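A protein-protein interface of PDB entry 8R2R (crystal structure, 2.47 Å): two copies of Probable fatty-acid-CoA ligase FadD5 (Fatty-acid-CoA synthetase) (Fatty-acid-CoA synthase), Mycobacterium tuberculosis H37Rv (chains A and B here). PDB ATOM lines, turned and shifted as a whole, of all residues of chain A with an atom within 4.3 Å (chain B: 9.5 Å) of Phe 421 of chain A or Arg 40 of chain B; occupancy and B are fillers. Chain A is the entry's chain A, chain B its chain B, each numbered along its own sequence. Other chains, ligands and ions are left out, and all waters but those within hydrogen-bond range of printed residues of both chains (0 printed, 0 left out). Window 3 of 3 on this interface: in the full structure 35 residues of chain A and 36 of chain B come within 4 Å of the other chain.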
ATOM      1  N   ALA A 403      -7.601 -19.031  23.993  1.00  0.00           N
ATOM      2  CA  ALA A 403      -8.746 -19.846  24.379  1.00  0.00           C
ATOM      3  C   ALA A 403      -9.372 -20.500  23.156  1.00  0.00           C
ATOM      4  O   ALA A 403      -9.401 -19.898  22.074  1.00  0.00           O
ATOM      5  CB  ALA A 403      -9.796 -19.001  25.109  1.00  0.00           C
ATOM      6  N   PRO A 404      -9.909 -21.715  23.290  1.00  0.00           N
ATOM      7  CA  PRO A 404     -10.628 -22.321  22.157  1.00  0.00           C
ATOM      8  C   PRO A 404     -11.854 -21.524  21.733  1.00  0.00           C
ATOM      9  O   PRO A 404     -12.252 -21.585  20.562  1.00  0.00           O
ATOM     10  CB  PRO A 404     -11.019 -23.711  22.684  1.00  0.00           C
ATOM     11  CG  PRO A 404     -10.212 -23.914  23.946  1.00  0.00           C
ATOM     12  CD  PRO A 404      -9.984 -22.548  24.502  1.00  0.00           C
ATOM     13  N   LEU A 406     -12.160 -18.375  21.296  1.00  0.00           N
ATOM     14  CA  LEU A 406     -11.905 -17.144  20.565  1.00  0.00           C
ATOM     15  C   LEU A 406     -12.408 -17.273  19.130  1.00  0.00           C
ATOM     16  O   LEU A 406     -12.556 -18.375  18.595  1.00  0.00           O
ATOM     17  CB  LEU A 406     -10.415 -16.807  20.569  1.00  0.00           C
ATOM     18  CG  LEU A 406      -9.838 -16.307  21.888  1.00  0.00           C
ATOM     19  CD1 LEU A 406      -8.330 -16.274  21.808  1.00  0.00           C
ATOM     20  CD2 LEU A 406     -10.385 -14.926  22.220  1.00  0.00           C
ATOM     21  N   MET A 407     -12.676 -16.126  18.508  1.00  0.00           N
ATOM     22  CA  MET A 407     -13.143 -16.117  17.128  1.00  0.00           C
ATOM     23  C   MET A 407     -12.095 -16.736  16.209  1.00  0.00           C
ATOM     24  O   MET A 407     -10.895 -16.703  16.490  1.00  0.00           O
ATOM     25  CB  MET A 407     -13.447 -14.691  16.670  1.00  0.00           C
ATOM     26  CG  MET A 407     -12.212 -13.825  16.561  1.00  0.00           C
ATOM     27  SD  MET A 407     -12.408 -12.442  15.434  1.00  0.00           S
ATOM     28  CE  MET A 407     -10.775 -11.720  15.525  1.00  0.00           C
ATOM     29  N   SER A 408     -12.563 -17.312  15.100  1.00  0.00           N
ATOM     30  CA  SER A 408     -11.647 -17.912  14.133  1.00  0.00           C
ATOM     31  C   SER A 408     -10.847 -16.845  13.400  1.00  0.00           C
ATOM     32  O   SER A 408      -9.621 -16.937  13.290  1.00  0.00           O
ATOM     33  CB  SER A 408     -12.422 -18.771  13.131  1.00  0.00           C
ATOM     34  OG  SER A 408     -13.066 -19.855  13.767  1.00  0.00           O
ATOM     35  N   THR A 417      -6.999  -9.886  11.068  1.00  0.00           N
ATOM     36  CA  THR A 417      -6.873 -11.085  11.892  1.00  0.00           C
ATOM     37  C   THR A 417      -5.463 -11.224  12.446  1.00  0.00           C
ATOM     38  O   THR A 417      -5.283 -11.587  13.615  1.00  0.00           O
ATOM     39  CB  THR A 417      -7.250 -12.331  11.087  1.00  0.00           C
ATOM     40  OG1 THR A 417      -8.563 -12.172  10.535  1.00  0.00           O
ATOM     41  CG2 THR A 417      -7.235 -13.562  11.977  1.00  0.00           C
ATOM     42  N   ALA A 418      -4.452 -10.938  11.624  1.00  0.00           N
ATOM     43  CA  ALA A 418      -3.076 -11.034  12.095  1.00  0.00           C
ATOM     44  C   ALA A 418      -2.774  -9.969  13.141  1.00  0.00           C
ATOM     45  O   ALA A 418      -2.144 -10.263  14.166  1.00  0.00           O
ATOM     46  CB  ALA A 418      -2.111 -10.933  10.917  1.00  0.00           C
ATOM     47  N   GLU A 419      -3.221  -8.727  12.910  1.00  0.00           N
ATOM     48  CA  GLU A 419      -3.044  -7.692  13.924  1.00  0.00           C
ATOM     49  C   GLU A 419      -3.749  -8.063  15.223  1.00  0.00           C
ATOM     50  O   GLU A 419      -3.216  -7.817  16.312  1.00  0.00           O
ATOM     51  CB  GLU A 419      -3.549  -6.343  13.410  1.00  0.00           C
ATOM     52  CG  GLU A 419      -3.112  -5.166  14.278  1.00  0.00           C
ATOM     53  CD  GLU A 419      -3.428  -3.817  13.655  1.00  0.00           C
ATOM     54  OE1 GLU A 419      -4.141  -3.784  12.630  1.00  0.00           O
ATOM     55  OE2 GLU A 419      -2.958  -2.789  14.190  1.00  0.00           O
ATOM     56  N   ALA A 420      -4.932  -8.675  15.131  1.00  0.00           N
ATOM     57  CA  ALA A 420      -5.672  -9.067  16.322  1.00  0.00           C
ATOM     58  C   ALA A 420      -5.007 -10.215  17.064  1.00  0.00           C
ATOM     59  O   ALA A 420      -5.197 -10.342  18.278  1.00  0.00           O
ATOM     60  CB  ALA A 420      -7.105  -9.450  15.948  1.00  0.00           C
ATOM     61  N   PHE A 421      -4.235 -11.051  16.367  1.00  0.00           N
ATOM     62  CA  PHE A 421      -3.556 -12.187  16.979  1.00  0.00           C
ATOM     63  C   PHE A 421      -2.043 -12.010  16.997  1.00  0.00           C
ATOM     64  O   PHE A 421      -1.307 -13.001  17.089  1.00  0.00           O
ATOM     65  CB  PHE A 421      -3.934 -13.485  16.261  1.00  0.00           C
ATOM     66  CG  PHE A 421      -5.345 -13.932  16.521  1.00  0.00           C
ATOM     67  CD1 PHE A 421      -5.670 -14.579  17.702  1.00  0.00           C
ATOM     68  CD2 PHE A 421      -6.348 -13.700  15.594  1.00  0.00           C
ATOM     69  CE1 PHE A 421      -6.965 -14.981  17.954  1.00  0.00           C
ATOM     70  CE2 PHE A 421      -7.646 -14.103  15.841  1.00  0.00           C
ATOM     71  CZ  PHE A 421      -7.953 -14.748  17.022  1.00  0.00           C
ATOM     72  N   ALA A 422      -1.567 -10.767  16.916  1.00  0.00           N
ATOM     73  CA  ALA A 422      -0.136 -10.499  16.895  1.00  0.00           C
ATOM     74  C   ALA A 422       0.554 -11.099  18.114  1.00  0.00           C
ATOM     75  O   ALA A 422       0.133 -10.880  19.253  1.00  0.00           O
ATOM     76  CB  ALA A 422       0.104  -8.996  16.840  1.00  0.00           C
ATOM     77  N   GLY A 423       1.616 -11.864  17.870  1.00  0.00           N
ATOM     78  CA  GLY A 423       2.378 -12.479  18.933  1.00  0.00           C
ATOM     79  C   GLY A 423       1.849 -13.807  19.420  1.00  0.00           C
ATOM     80  O   GLY A 423       2.427 -14.377  20.352  1.00  0.00           O
ATOM     81  N   GLY A 424       0.772 -14.318  18.829  1.00  0.00           N
ATOM     82  CA  GLY A 424       0.194 -15.584  19.230  1.00  0.00           C
ATOM     83  C   GLY A 424      -0.943 -15.493  20.226  1.00  0.00           C
ATOM     84  O   GLY A 424      -1.415 -16.534  20.702  1.00  0.00           O
ATOM     85  N   TRP A 425      -1.384 -14.288  20.566  1.00  0.00           N
ATOM     86  CA  TRP A 425      -2.452 -14.079  21.529  1.00  0.00           C
ATOM     87  C   TRP A 425      -3.430 -13.056  20.965  1.00  0.00           C
ATOM     88  O   TRP A 425      -3.058 -12.197  20.162  1.00  0.00           O
ATOM     89  CB  TRP A 425      -1.898 -13.604  22.892  1.00  0.00           C
ATOM     90  CG  TRP A 425      -0.946 -14.575  23.556  1.00  0.00           C
ATOM     91  CD1 TRP A 425       0.330 -14.874  23.164  1.00  0.00           C
ATOM     92  CD2 TRP A 425      -1.190 -15.349  24.740  1.00  0.00           C
ATOM     93  NE1 TRP A 425       0.887 -15.793  24.021  1.00  0.00           N
ATOM     94  CE2 TRP A 425      -0.023 -16.100  24.997  1.00  0.00           C
ATOM     95  CE3 TRP A 425      -2.281 -15.484  25.604  1.00  0.00           C
ATOM     96  CZ2 TRP A 425       0.081 -16.971  26.080  1.00  0.00           C
ATOM     97  CZ3 TRP A 425      -2.173 -16.355  26.681  1.00  0.00           C
ATOM     98  CH2 TRP A 425      -1.000 -17.086  26.907  1.00  0.00           C
ATOM     99  N   PHE A 426      -4.690 -13.161  21.379  1.00  0.00           N
ATOM    100  CA  PHE A 426      -5.708 -12.236  20.903  1.00  0.00           C
ATOM    101  C   PHE A 426      -5.657 -10.935  21.700  1.00  0.00           C
ATOM    102  O   PHE A 426      -5.610 -10.952  22.932  1.00  0.00           O
ATOM    103  CB  PHE A 426      -7.097 -12.866  20.998  1.00  0.00           C
ATOM    104  CG  PHE A 426      -8.209 -11.895  20.746  1.00  0.00           C
ATOM    105  CD1 PHE A 426      -8.522 -11.500  19.454  1.00  0.00           C
ATOM    106  CD2 PHE A 426      -8.934 -11.363  21.800  1.00  0.00           C
ATOM    107  CE1 PHE A 426      -9.540 -10.592  19.216  1.00  0.00           C
ATOM    108  CE2 PHE A 426      -9.956 -10.460  21.570  1.00  0.00           C
ATOM    109  CZ  PHE A 426     -10.259 -10.071  20.272  1.00  0.00           C
ATOM    110  N   TYR B  37      -3.571 -23.671  25.372  1.00  0.00           N
ATOM    111  CA  TYR B  37      -4.784 -23.778  24.566  1.00  0.00           C
ATOM    112  C   TYR B  37      -4.483 -23.507  23.092  1.00  0.00           C
ATOM    113  O   TYR B  37      -5.381 -23.191  22.311  1.00  0.00           O
ATOM    114  CB  TYR B  37      -5.862 -22.821  25.090  1.00  0.00           C
ATOM    115  CG  TYR B  37      -6.688 -23.403  26.219  1.00  0.00           C
ATOM    116  CD1 TYR B  37      -7.058 -24.746  26.209  1.00  0.00           C
ATOM    117  CD2 TYR B  37      -7.091 -22.619  27.296  1.00  0.00           C
ATOM    118  CE1 TYR B  37      -7.813 -25.295  27.236  1.00  0.00           C
ATOM    119  CE2 TYR B  37      -7.850 -23.161  28.334  1.00  0.00           C
ATOM    120  CZ  TYR B  37      -8.209 -24.502  28.298  1.00  0.00           C
ATOM    121  OH  TYR B  37      -8.959 -25.063  29.319  1.00  0.00           O
ATOM    122  N   LEU B  38      -3.211 -23.655  22.727  1.00  0.00           N
ATOM    123  CA  LEU B  38      -2.770 -23.413  21.361  1.00  0.00           C
ATOM    124  C   LEU B  38      -3.373 -24.440  20.402  1.00  0.00           C
ATOM    125  O   LEU B  38      -3.716 -25.562  20.786  1.00  0.00           O
ATOM    126  CB  LEU B  38      -1.241 -23.438  21.290  1.00  0.00           C
ATOM    127  CG  LEU B  38      -0.566 -22.643  20.170  1.00  0.00           C
ATOM    128  CD1 LEU B  38      -1.133 -21.229  20.076  1.00  0.00           C
ATOM    129  CD2 LEU B  38       0.943 -22.606  20.385  1.00  0.00           C
ATOM    130  N   ALA B  39      -3.503 -24.030  19.137  1.00  0.00           N
ATOM    131  CA  ALA B  39      -4.216 -24.720  18.061  1.00  0.00           C
ATOM    132  C   ALA B  39      -5.706 -24.905  18.348  1.00  0.00           C
ATOM    133  O   ALA B  39      -6.372 -25.666  17.635  1.00  0.00           O
ATOM    134  CB  ALA B  39      -3.582 -26.075  17.722  1.00  0.00           C
ATOM    135  N   ARG B  40      -6.248 -24.221  19.366  1.00  0.00           N
ATOM    136  CA  ARG B  40      -7.680 -24.264  19.695  1.00  0.00           C
ATOM    137  C   ARG B  40      -8.122 -25.661  20.137  1.00  0.00           C
ATOM    138  O   ARG B  40      -9.233 -26.108  19.836  1.00  0.00           O
ATOM    139  CB  ARG B  40      -8.540 -23.773  18.522  1.00  0.00           C
ATOM    140  CG  ARG B  40      -8.329 -22.315  18.145  1.00  0.00           C
ATOM    141  CD  ARG B  40      -9.393 -21.410  18.751  1.00  0.00           C
ATOM    142  NE  ARG B  40      -9.043 -20.001  18.619  1.00  0.00           N
ATOM    143  CZ  ARG B  40      -9.229 -19.279  17.522  1.00  0.00           C
ATOM    144  NH1 ARG B  40      -9.778 -19.797  16.437  1.00  0.00           N
ATOM    145  NH2 ARG B  40      -8.847 -18.005  17.513  1.00  0.00           N
ATOM    146  N   ARG B  41      -7.249 -26.360  20.860  1.00  0.00           N
ATOM    147  CA  ARG B  41      -7.538 -27.703  21.342  1.00  0.00           C
ATOM    148  C   ARG B  41      -8.126 -27.641  22.746  1.00  0.00           C
ATOM    149  O   ARG B  41      -7.703 -26.827  23.572  1.00  0.00           O
ATOM    150  CB  ARG B  41      -6.278 -28.571  21.352  1.00  0.00           C
ATOM    151  CG  ARG B  41      -5.520 -28.615  20.035  1.00  0.00           C
ATOM    152  CD  ARG B  41      -6.438 -28.930  18.863  1.00  0.00           C
ATOM    153  NE  ARG B  41      -5.676 -29.233  17.657  1.00  0.00           N
ATOM    154  CZ  ARG B  41      -6.210 -29.587  16.496  1.00  0.00           C
ATOM    155  NH1 ARG B  41      -7.522 -29.650  16.327  1.00  0.00           N
ATOM    156  NH2 ARG B  41      -5.407 -29.896  15.480  1.00  0.00           N
ATOM    157  N   GLN B  42      -9.102 -28.506  23.013  1.00  0.00           N
ATOM    158  CA  GLN B  42      -9.673 -28.662  24.349  1.00  0.00           C
ATOM    159  C   GLN B  42      -9.431 -30.094  24.819  1.00  0.00           C
ATOM    160  O   GLN B  42     -10.013 -31.038  24.275  1.00  0.00           O
ATOM    161  CB  GLN B  42     -11.164 -28.315  24.363  1.00  0.00           C
ATOM    162  CG  GLN B  42     -11.837 -28.425  25.741  1.00  0.00           C
ATOM    163  CD  GLN B  42     -11.270 -27.457  26.773  1.00  0.00           C
ATOM    164  OE1 GLN B  42     -10.175 -27.659  27.300  1.00  0.00           O
ATOM    165  NE2 GLN B  42     -12.024 -26.402  27.072  1.00  0.00           N
ATOM    166  N   ASN B  43      -8.559 -30.248  25.815  1.00  0.00           N
ATOM    167  CA  ASN B  43      -8.317 -31.525  26.475  1.00  0.00           C
ATOM    168  C   ASN B  43      -7.671 -31.235  27.820  1.00  0.00           C
ATOM    169  O   ASN B  43      -7.203 -30.123  28.067  1.00  0.00           O
ATOM    170  CB  ASN B  43      -7.435 -32.451  25.634  1.00  0.00           C
ATOM    171  CG  ASN B  43      -6.161 -31.780  25.176  1.00  0.00           C
ATOM    172  OD1 ASN B  43      -5.255 -31.540  25.975  1.00  0.00           O
ATOM    173  ND2 ASN B  43      -6.078 -31.479  23.881  1.00  0.00           N
ATOM    174  N   ASN B  46      -4.079 -29.545  27.880  1.00  0.00           N
ATOM    175  CA  ASN B  46      -4.088 -28.090  27.734  1.00  0.00           C
ATOM    176  C   ASN B  46      -4.622 -27.406  28.986  1.00  0.00           C
ATOM    177  O   ASN B  46      -4.109 -26.358  29.395  1.00  0.00           O
ATOM    178  CB  ASN B  46      -4.926 -27.679  26.523  1.00  0.00           C
ATOM    179  CG  ASN B  46      -4.210 -27.895  25.212  1.00  0.00           C
ATOM    180  OD1 ASN B  46      -3.213 -28.612  25.140  1.00  0.00           O
ATOM    181  ND2 ASN B  46      -4.723 -27.274  24.158  1.00  0.00           N
ATOM    182  N   ASP B 195       0.581 -31.510  18.751  1.00  0.00           N
ATOM    183  CA  ASP B 195      -0.780 -31.116  18.419  1.00  0.00           C
ATOM    184  C   ASP B 195      -1.719 -32.291  18.652  1.00  0.00           C
ATOM    185  O   ASP B 195      -1.585 -33.338  18.011  1.00  0.00           O
ATOM    186  CB  ASP B 195      -0.859 -30.643  16.972  1.00  0.00           C
ATOM    187  CG  ASP B 195      -2.252 -30.211  16.588  1.00  0.00           C
ATOM    188  OD1 ASP B 195      -2.808 -29.327  17.278  1.00  0.00           O
ATOM    189  OD2 ASP B 195      -2.794 -30.759  15.605  1.00  0.00           O
ATOM    190  N   ILE B 196      -2.667 -32.120  19.566  1.00  0.00           N
ATOM    191  CA  ILE B 196      -3.589 -33.189  19.933  1.00  0.00           C
ATOM    192  C   ILE B 196      -4.996 -32.820  19.478  1.00  0.00           C
ATOM    193  O   ILE B 196      -5.711 -32.095  20.188  1.00  0.00           O
ATOM    194  CB  ILE B 196      -3.548 -33.457  21.443  1.00  0.00           C
ATOM    195  CG1 ILE B 196      -2.128 -33.829  21.865  1.00  0.00           C
ATOM    196  CG2 ILE B 196      -4.548 -34.550  21.821  1.00  0.00           C
ATOM    197  CD1 ILE B 196      -1.898 -33.725  23.357  1.00  0.00           C
ATOM    198  N   PRO B 197      -5.426 -33.289  18.308  1.00  0.00           N
ATOM    199  CA  PRO B 197      -6.799 -33.023  17.867  1.00  0.00           C
ATOM    200  C   PRO B 197      -7.800 -33.593  18.854  1.00  0.00           C
ATOM    201  O   PRO B 197      -7.577 -34.643  19.459  1.00  0.00           O
ATOM    202  CB  PRO B 197      -6.884 -33.740  16.514  1.00  0.00           C
ATOM    203  CG  PRO B 197      -5.466 -33.869  16.060  1.00  0.00           C
ATOM    204  CD  PRO B 197      -4.657 -34.047  17.309  1.00  0.00           C
ATOM    205  N   ASN B 198      -8.926 -32.891  19.000  1.00  0.00           N
ATOM    206  CA  ASN B 198      -9.920 -33.257  20.002  1.00  0.00           C
ATOM    207  C   ASN B 198     -10.581 -34.606  19.737  1.00  0.00           C
ATOM    208  O   ASN B 198     -11.225 -35.145  20.645  1.00  0.00           O
ATOM    209  CB  ASN B 198     -10.986 -32.167  20.099  1.00  0.00           C
ATOM    210  CG  ASN B 198     -10.410 -30.829  20.532  1.00  0.00           C
ATOM    211  OD1 ASN B 198      -9.341 -30.760  21.145  1.00  0.00           O
ATOM    212  ND2 ASN B 198     -11.117 -29.757  20.211  1.00  0.00           N
ATOM    213  N   ASP B 199     -10.445 -35.163  18.533  1.00  0.00           N
ATOM    214  CA  ASP B 199     -10.947 -36.499  18.234  1.00  0.00           C
ATOM    215  C   ASP B 199      -9.921 -37.586  18.503  1.00  0.00           C
ATOM    216  O   ASP B 199     -10.184 -38.756  18.203  1.00  0.00           O
ATOM    217  CB  ASP B 199     -11.394 -36.594  16.774  1.00  0.00           C
ATOM    218  CG  ASP B 199     -12.634 -35.787  16.493  1.00  0.00           C
ATOM    219  OD1 ASP B 199     -13.504 -35.700  17.389  1.00  0.00           O
ATOM    220  OD2 ASP B 199     -12.737 -35.239  15.373  1.00  0.00           O
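The backbone carbonyl oxygen (O) of Met 407 of chain A sits at hydrogen-bond distance from the guanidinium group (NH2) of Arg 40 of chain B, 2.6 Å away. The backbone carbonyl oxygen (O) of Ala 403 of chain A sits at hydrogen-bond distance from the guanidinium group (NE) of Arg 40 of chain B (3.5 Å).
The backbone carbonyl oxygen (O) of Arg 41 of chain B is in hydrogen-bond range of the side-chain amide nitrogen (ND2) of Asn 46 of chain B. NH2 of Arg 41 of chain B is in salt-bridge range of OD2 of Asp 195 of chain B, 2.8 Å away.
CD of Pro 404 of chain A touches CG of Tyr 37 of chain B, 3.8 Å away. Pro 404 of chain A touches Arg 40 of chain B. Arg 41 of chain B touches Pro 404 of chain A. CZ of Arg 40 of chain B touches O of Leu 406 of chain A, at 3.6 Å. Arg 40 of chain B touches Ser 408 of chain A. Arg 40 of chain B touches Phe 421 of chain A.
Of chain B, only Arg 40 comes within 4 Å of Phe 421 of chain A. Of chain A, only Ala 403, Pro 404, Leu 406, Met 407, Ser 408 and Phe 421 come within 4 Å of Arg 40 of chain B. Of the printed residues of chain B, Ser 408 of chain A touches Arg 40 (3.5 Å). No residue of chain B comes within 4 Å of Ala 420 of chain A. No residue of chain B comes within 4 Å of Ala 422 of chain A. No residue of chain B comes within 4 Å of Gly 423 of chain A. No residue of chain B comes within 4 Å of Gly 424 of chain A. Printed residues of chain B within 4 Å of Ala 403 of chain A: Arg 40. Of the printed residues of chain A, Tyr 37 of chain B touches Pro 404. Printed residues of chain B within 4 Å of Pro 404 of chain A: Tyr 37, Arg 40 and Arg 41. Of the printed residues of chain B, Met 407 of chain A touches Arg 40 (2.6 Å). Of the printed residues of chain B, Leu 406 of chain A touches Arg 40. Trp 425 of chain A touches none of the printed residues of chain B. The nearest residue of chain B that does not touch Phe 421 of chain A is Leu 38 of chain B (8.4 Å).
Of the 15 printed residues of chain A, 6 touch a printed residue of chain B. Hydrophobic or aromatic side chains of chain A within 4 Å of the printed part of chain B: Pro 404, Leu 406 and Phe 421. Of the 13 printed residues of chain B, 3 touch a printed residue of chain A. Printed residues of chain B that touch a printed residue of chain A: Tyr 37, Arg 40 and Arg 41. Hydrophobic or aromatic side chains of chain B that line the printed part of chain A: Tyr 37.
No position is printed for both chains.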
